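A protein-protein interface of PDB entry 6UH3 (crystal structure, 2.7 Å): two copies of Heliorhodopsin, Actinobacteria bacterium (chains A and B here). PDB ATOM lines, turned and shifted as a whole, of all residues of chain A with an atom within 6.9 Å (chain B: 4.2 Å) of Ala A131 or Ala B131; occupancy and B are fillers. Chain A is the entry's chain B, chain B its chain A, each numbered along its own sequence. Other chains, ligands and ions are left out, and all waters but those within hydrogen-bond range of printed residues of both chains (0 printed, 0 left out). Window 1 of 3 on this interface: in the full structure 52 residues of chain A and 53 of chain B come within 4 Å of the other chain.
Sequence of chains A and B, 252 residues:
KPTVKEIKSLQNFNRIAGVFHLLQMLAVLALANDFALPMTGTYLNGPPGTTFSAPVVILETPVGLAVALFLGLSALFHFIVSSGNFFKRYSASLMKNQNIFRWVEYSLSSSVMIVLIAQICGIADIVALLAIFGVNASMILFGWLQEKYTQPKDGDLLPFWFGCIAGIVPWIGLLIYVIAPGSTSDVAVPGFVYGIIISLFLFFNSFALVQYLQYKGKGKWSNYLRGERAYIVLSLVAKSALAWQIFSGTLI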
ATOM      1  N   ASP A 125     -15.141   1.073  14.249  1.00  0.00           N
ATOM      2  CA  ASP A 125     -13.933   0.746  14.988  1.00  0.00           C
ATOM      3  C   ASP A 125     -12.711   1.000  14.113  1.00  0.00           C
ATOM      4  O   ASP A 125     -12.536   0.360  13.072  1.00  0.00           O
ATOM      5  CB  ASP A 125     -13.972  -0.708  15.445  1.00  0.00           C
ATOM      6  CG  ASP A 125     -12.817  -1.047  16.343  1.00  0.00           C
ATOM      7  OD1 ASP A 125     -11.669  -1.113  15.859  1.00  0.00           O
ATOM      8  OD2 ASP A 125     -13.054  -1.240  17.548  1.00  0.00           O
ATOM      9  N   ILE A 126     -11.845   1.906  14.577  1.00  0.00           N
ATOM     10  CA  ILE A 126     -10.648   2.313  13.839  1.00  0.00           C
ATOM     11  C   ILE A 126      -9.743   1.145  13.478  1.00  0.00           C
ATOM     12  O   ILE A 126      -9.024   1.198  12.470  1.00  0.00           O
ATOM     13  CB  ILE A 126      -9.864   3.352  14.661  1.00  0.00           C
ATOM     14  CG1 ILE A 126      -8.806   4.018  13.795  1.00  0.00           C
ATOM     15  CG2 ILE A 126      -9.202   2.714  15.880  1.00  0.00           C
ATOM     16  CD1 ILE A 126      -8.264   5.245  14.418  1.00  0.00           C
ATOM     17  N   VAL A 127      -9.741   0.088  14.286  1.00  0.00           N
ATOM     18  CA  VAL A 127      -8.884  -1.052  13.989  1.00  0.00           C
ATOM     19  C   VAL A 127      -9.526  -1.923  12.929  1.00  0.00           C
ATOM     20  O   VAL A 127      -8.846  -2.454  12.041  1.00  0.00           O
ATOM     21  CB  VAL A 127      -8.603  -1.842  15.273  1.00  0.00           C
ATOM     22  CG1 VAL A 127      -7.882  -3.127  14.950  1.00  0.00           C
ATOM     23  CG2 VAL A 127      -7.785  -1.003  16.239  1.00  0.00           C
ATOM     24  N   ALA A 128     -10.850  -2.068  13.006  1.00  0.00           N
ATOM     25  CA  ALA A 128     -11.589  -2.775  11.971  1.00  0.00           C
ATOM     26  C   ALA A 128     -11.345  -2.128  10.627  1.00  0.00           C
ATOM     27  O   ALA A 128     -11.085  -2.809   9.632  1.00  0.00           O
ATOM     28  CB  ALA A 128     -13.082  -2.768  12.290  1.00  0.00           C
ATOM     29  N   LEU A 129     -11.452  -0.803  10.579  1.00  0.00           N
ATOM     30  CA  LEU A 129     -11.314  -0.104   9.311  1.00  0.00           C
ATOM     31  C   LEU A 129      -9.861  -0.157   8.842  1.00  0.00           C
ATOM     32  O   LEU A 129      -9.593  -0.346   7.651  1.00  0.00           O
ATOM     33  CB  LEU A 129     -11.822   1.329   9.475  1.00  0.00           C
ATOM     34  CG  LEU A 129     -13.332   1.410   9.779  1.00  0.00           C
ATOM     35  CD1 LEU A 129     -13.740   2.834  10.131  1.00  0.00           C
ATOM     36  CD2 LEU A 129     -14.177   0.878   8.637  1.00  0.00           C
ATOM     37  N   LEU A 130      -8.914  -0.060   9.782  1.00  0.00           N
ATOM     38  CA  LEU A 130      -7.498  -0.243   9.459  1.00  0.00           C
ATOM     39  C   LEU A 130      -7.247  -1.619   8.856  1.00  0.00           C
ATOM     40  O   LEU A 130      -6.542  -1.759   7.848  1.00  0.00           O
ATOM     41  CB  LEU A 130      -6.643  -0.071  10.713  1.00  0.00           C
ATOM     42  CG  LEU A 130      -5.150  -0.344  10.493  1.00  0.00           C
ATOM     43  CD1 LEU A 130      -4.558   0.688   9.539  1.00  0.00           C
ATOM     44  CD2 LEU A 130      -4.372  -0.412  11.799  1.00  0.00           C
ATOM     45  N   ALA A 131      -7.771  -2.656   9.514  1.00  0.00           N
ATOM     46  CA  ALA A 131      -7.570  -4.032   9.065  1.00  0.00           C
ATOM     47  C   ALA A 131      -8.263  -4.317   7.730  1.00  0.00           C
ATOM     48  O   ALA A 131      -7.675  -4.956   6.848  1.00  0.00           O
ATOM     49  CB  ALA A 131      -8.042  -4.999  10.145  1.00  0.00           C
ATOM     50  N   ILE A 132      -9.525  -3.884   7.572  1.00  0.00           N
ATOM     51  CA  ILE A 132     -10.232  -4.061   6.295  1.00  0.00           C
ATOM     52  C   ILE A 132      -9.411  -3.482   5.157  1.00  0.00           C
ATOM     53  O   ILE A 132      -9.270  -4.091   4.086  1.00  0.00           O
ATOM     54  CB  ILE A 132     -11.619  -3.395   6.315  1.00  0.00           C
ATOM     55  CG1 ILE A 132     -12.604  -4.116   7.228  1.00  0.00           C
ATOM     56  CG2 ILE A 132     -12.180  -3.353   4.897  1.00  0.00           C
ATOM     57  CD1 ILE A 132     -13.854  -3.278   7.498  1.00  0.00           C
ATOM     58  N   PHE A 133      -8.884  -2.273   5.372  1.00  0.00           N
ATOM     59  CA  PHE A 133      -8.027  -1.654   4.376  1.00  0.00           C
ATOM     60  C   PHE A 133      -6.855  -2.570   4.081  1.00  0.00           C
ATOM     61  O   PHE A 133      -6.590  -2.913   2.923  1.00  0.00           O
ATOM     62  CB  PHE A 133      -7.521  -0.308   4.896  1.00  0.00           C
ATOM     63  CG  PHE A 133      -6.757   0.492   3.879  1.00  0.00           C
ATOM     64  CD1 PHE A 133      -7.252   1.710   3.438  1.00  0.00           C
ATOM     65  CD2 PHE A 133      -5.563   0.035   3.357  1.00  0.00           C
ATOM     66  CE1 PHE A 133      -6.563   2.465   2.503  1.00  0.00           C
ATOM     67  CE2 PHE A 133      -4.874   0.768   2.414  1.00  0.00           C
ATOM     68  CZ  PHE A 133      -5.377   1.993   1.991  1.00  0.00           C
ATOM     69  N   GLY A 134      -6.175  -3.008   5.145  1.00  0.00           N
ATOM     70  CA  GLY A 134      -5.014  -3.869   4.993  1.00  0.00           C
ATOM     71  C   GLY A 134      -5.318  -5.147   4.233  1.00  0.00           C
ATOM     72  O   GLY A 134      -4.586  -5.531   3.318  1.00  0.00           O
ATOM     73  N   VAL A 135      -6.419  -5.816   4.578  1.00  0.00           N
ATOM     74  CA  VAL A 135      -6.677  -7.089   3.915  1.00  0.00           C
ATOM     75  C   VAL A 135      -7.118  -6.875   2.466  1.00  0.00           C
ATOM     76  O   VAL A 135      -6.809  -7.699   1.594  1.00  0.00           O
ATOM     77  CB  VAL A 135      -7.674  -7.925   4.751  1.00  0.00           C
ATOM     78  CG1 VAL A 135      -9.085  -7.404   4.621  1.00  0.00           C
ATOM     79  CG2 VAL A 135      -7.604  -9.374   4.326  1.00  0.00           C
ATOM     80  N   ASN A 136      -7.801  -5.760   2.173  1.00  0.00           N
ATOM     81  CA  ASN A 136      -8.167  -5.441   0.795  1.00  0.00           C
ATOM     82  C   ASN A 136      -6.915  -5.192  -0.042  1.00  0.00           C
ATOM     83  O   ASN A 136      -6.834  -5.616  -1.201  1.00  0.00           O
ATOM     84  CB  ASN A 136      -9.105  -4.232   0.761  1.00  0.00           C
ATOM     85  CG  ASN A 136      -9.666  -3.956  -0.626  1.00  0.00           C
ATOM     86  OD1 ASN A 136     -10.616  -4.603  -1.062  1.00  0.00           O
ATOM     87  ND2 ASN A 136      -9.102  -2.973  -1.307  1.00  0.00           N
ATOM     88  N   ALA A 137      -5.931  -4.486   0.524  1.00  0.00           N
ATOM     89  CA  ALA A 137      -4.647  -4.325  -0.155  1.00  0.00           C
ATOM     90  C   ALA A 137      -3.984  -5.677  -0.420  1.00  0.00           C
ATOM     91  O   ALA A 137      -3.445  -5.907  -1.511  1.00  0.00           O
ATOM     92  CB  ALA A 137      -3.724  -3.431   0.673  1.00  0.00           C
ATOM     93  N   VAL A 169     -13.142 -11.601   2.884  1.00  0.00           N
ATOM     94  CA  VAL A 169     -13.177 -11.248   4.310  1.00  0.00           C
ATOM     95  C   VAL A 169     -13.881  -9.915   4.577  1.00  0.00           C
ATOM     96  O   VAL A 169     -14.657  -9.835   5.545  1.00  0.00           O
ATOM     97  CB  VAL A 169     -11.754 -11.255   4.907  1.00  0.00           C
ATOM     98  CG1 VAL A 169     -11.756 -10.623   6.281  1.00  0.00           C
ATOM     99  CG2 VAL A 169     -11.210 -12.673   4.996  1.00  0.00           C
ATOM    100  N   PRO A 170     -13.673  -8.858   3.773  1.00  0.00           N
ATOM    101  CA  PRO A 170     -14.360  -7.589   4.062  1.00  0.00           C
ATOM    102  C   PRO A 170     -15.857  -7.691   3.888  1.00  0.00           C
ATOM    103  O   PRO A 170     -16.638  -7.140   4.676  1.00  0.00           O
ATOM    104  CB  PRO A 170     -13.770  -6.655   3.009  1.00  0.00           C
ATOM    105  CG  PRO A 170     -12.404  -7.094   2.844  1.00  0.00           C
ATOM    106  CD  PRO A 170     -12.364  -8.584   3.151  1.00  0.00           C
ATOM    107  N   VAL B 127     -15.895  -7.310  13.613  1.00  0.00           N
ATOM    108  CA  VAL B 127     -15.350  -7.164  12.270  1.00  0.00           C
ATOM    109  C   VAL B 127     -13.856  -6.991  12.345  1.00  0.00           C
ATOM    110  O   VAL B 127     -13.107  -7.574  11.550  1.00  0.00           O
ATOM    111  CB  VAL B 127     -16.004  -5.988  11.524  1.00  0.00           C
ATOM    112  CG1 VAL B 127     -15.268  -5.743  10.223  1.00  0.00           C
ATOM    113  CG2 VAL B 127     -17.473  -6.264  11.255  1.00  0.00           C
ATOM    114  N   ALA B 128     -13.409  -6.178  13.303  1.00  0.00           N
ATOM    115  CA  ALA B 128     -11.986  -5.976  13.514  1.00  0.00           C
ATOM    116  C   ALA B 128     -11.280  -7.308  13.687  1.00  0.00           C
ATOM    117  O   ALA B 128     -10.277  -7.585  13.020  1.00  0.00           O
ATOM    118  CB  ALA B 128     -11.753  -5.086  14.737  1.00  0.00           C
ATOM    119  N   LEU B 129     -11.792  -8.141  14.596  1.00  0.00           N
ATOM    120  CA  LEU B 129     -11.138  -9.409  14.890  1.00  0.00           C
ATOM    121  C   LEU B 129     -11.134 -10.323  13.666  1.00  0.00           C
ATOM    122  O   LEU B 129     -10.103 -10.927  13.334  1.00  0.00           O
ATOM    123  CB  LEU B 129     -11.859 -10.071  16.057  1.00  0.00           C
ATOM    124  CG  LEU B 129     -11.742  -9.285  17.370  1.00  0.00           C
ATOM    125  CD1 LEU B 129     -12.649  -9.836  18.457  1.00  0.00           C
ATOM    126  CD2 LEU B 129     -10.311  -9.272  17.849  1.00  0.00           C
ATOM    127  N   LEU B 130     -12.259 -10.375  12.943  1.00  0.00           N
ATOM    128  CA  LEU B 130     -12.326 -11.121  11.688  1.00  0.00           C
ATOM    129  C   LEU B 130     -11.267 -10.658  10.700  1.00  0.00           C
ATOM    130  O   LEU B 130     -10.485 -11.462  10.180  1.00  0.00           O
ATOM    131  CB  LEU B 130     -13.708 -10.956  11.065  1.00  0.00           C
ATOM    132  CG  LEU B 130     -13.811 -11.484   9.625  1.00  0.00           C
ATOM    133  CD1 LEU B 130     -13.611 -12.991   9.562  1.00  0.00           C
ATOM    134  CD2 LEU B 130     -15.119 -11.083   8.981  1.00  0.00           C
ATOM    135  N   ALA B 131     -11.237  -9.351  10.429  1.00  0.00           N
ATOM    136  CA  ALA B 131     -10.313  -8.798   9.445  1.00  0.00           C
ATOM    137  C   ALA B 131      -8.859  -9.022   9.846  1.00  0.00           C
ATOM    138  O   ALA B 131      -8.013  -9.320   8.990  1.00  0.00           O
ATOM    139  CB  ALA B 131     -10.596  -7.311   9.245  1.00  0.00           C
ATOM    140  N   ILE B 132      -8.548  -8.859  11.139  1.00  0.00           N
ATOM    141  CA  ILE B 132      -7.195  -9.129  11.624  1.00  0.00           C
ATOM    142  C   ILE B 132      -6.812 -10.568  11.343  1.00  0.00           C
ATOM    143  O   ILE B 132      -5.680 -10.868  10.947  1.00  0.00           O
ATOM    144  CB  ILE B 132      -7.091  -8.829  13.128  1.00  0.00           C
ATOM    145  CG1 ILE B 132      -7.194  -7.337  13.394  1.00  0.00           C
ATOM    146  CG2 ILE B 132      -5.787  -9.381  13.689  1.00  0.00           C
ATOM    147  CD1 ILE B 132      -7.439  -7.020  14.857  1.00  0.00           C
ATOM    148  N   PHE B 133      -7.732 -11.485  11.608  1.00  0.00           N
ATOM    149  CA  PHE B 133      -7.484 -12.880  11.299  1.00  0.00           C
ATOM    150  C   PHE B 133      -7.168 -13.029   9.816  1.00  0.00           C
ATOM    151  O   PHE B 133      -6.210 -13.711   9.435  1.00  0.00           O
ATOM    152  CB  PHE B 133      -8.710 -13.695  11.717  1.00  0.00           C
ATOM    153  CG  PHE B 133      -8.500 -15.168  11.700  1.00  0.00           C
ATOM    154  CD1 PHE B 133      -8.356 -15.861  12.889  1.00  0.00           C
ATOM    155  CD2 PHE B 133      -8.385 -15.852  10.504  1.00  0.00           C
ATOM    156  CE1 PHE B 133      -8.152 -17.216  12.894  1.00  0.00           C
ATOM    157  CE2 PHE B 133      -8.169 -17.209  10.496  1.00  0.00           C
ATOM    158  CZ  PHE B 133      -8.050 -17.895  11.693  1.00  0.00           C
ATOM    159  N   GLY B 134      -7.980 -12.389   8.971  1.00  0.00           N
ATOM    160  CA  GLY B 134      -7.773 -12.442   7.530  1.00  0.00           C
ATOM    161  C   GLY B 134      -6.436 -11.865   7.094  1.00  0.00           C
ATOM    162  O   GLY B 134      -5.712 -12.472   6.296  1.00  0.00           O
ATOM    163  N   VAL B 135      -6.082 -10.685   7.613  1.00  0.00           N
ATOM    164  CA  VAL B 135      -4.856 -10.074   7.118  1.00  0.00           C
ATOM    165  C   VAL B 135      -3.628 -10.787   7.673  1.00  0.00           C
ATOM    166  O   VAL B 135      -2.602 -10.893   6.984  1.00  0.00           O
ATOM    167  CB  VAL B 135      -4.862  -8.563   7.426  1.00  0.00           C
ATOM    168  CG1 VAL B 135      -4.487  -8.275   8.879  1.00  0.00           C
ATOM    169  CG2 VAL B 135      -3.923  -7.847   6.484  1.00  0.00           C
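OD1 of Asp A125 sits at hydrogen-bond distance from N of Val A127. OD1 of Asp A125 lies within hydrogen-bond range of N of Ala A128 (3.1 Å).
Ile B132 touches Val A127. N of Ala B128 touches CB of Ala A128, at 3.6 Å. Ala B131 touches Ala A131. Ile A132 touches Val B127 (CD1 to CG1, 3.9 Å). CB of Ala B131 touches N of Ile A132, 3.96 Å away. Val B135 touches Gly A134. Val A135 touches Gly B134. Val A135 touches Val B135 (N to CG2, 3.7 Å). CD2 of Leu B130 touches O of Val A169, at 3.7 Å. Ala B131 touches Val A169.
Of the printed residues of chain B, Val A127 touches Ile B132. Of the printed residues of chain B, Ala A131 touches Ala B131. Of the printed residues of chain B, Gly A134 touches Val B135 (3.8 Å). Of the printed residues of chain B, Val A135 touches Gly B134 and Val B135. Printed residues of chain A within 4 Å of Val B127: Ile A132. Of the printed residues of chain A, Ile B132 touches Val A127 (3.9 Å). The nearest residue of chain A that does not touch Ala B131 is Val A135 (4.5 Å). The nearest printed residue of chain B that does not touch Val A127 is Ala B128 (4.3 Å).
Of the 9 printed residues of chain B, 7 touch a printed residue of chain A. Hydrophobic or aromatic side chains of chain B that line the printed part of chain A: Val B127, Ala B128, Leu B130, Ala B131, Ile B132 and Val B135. Printed residues of chain A that touch a printed residue of chain B: Val A127, Ala A128, Ala A131, Ile A132, Gly A134, Val A135 and Val A169. Hydrophobic or aromatic side chains of chain A within 4 Å of the printed part of chain B: Val A127, Ala A128, Ala A131, Ile A132, Val A135 and Val A169. Among the printed residues, no Asp or Glu carboxylate lies within 4 Å of a Lys or Arg side-chain nitrogen of the other chain.
Val A127 touches Ile B132, and with the chains exchanged Ile A132 touches Val B127. Ala A128 touches its own counterpart, Ala B128. Ile A132 touches Ala B131, but with the chains exchanged Ala A131 does not touch Ile B132 (4.02 Å). Val B135 touches its own counterpart, Val A135. Positions printed for both chains: 127, 128, 129, 130, 131, 132, 133, 134 and 135. Of the 10 pairs that touch across the chains among the printed residues, 7 have their exchanged pair printed and touching as well.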
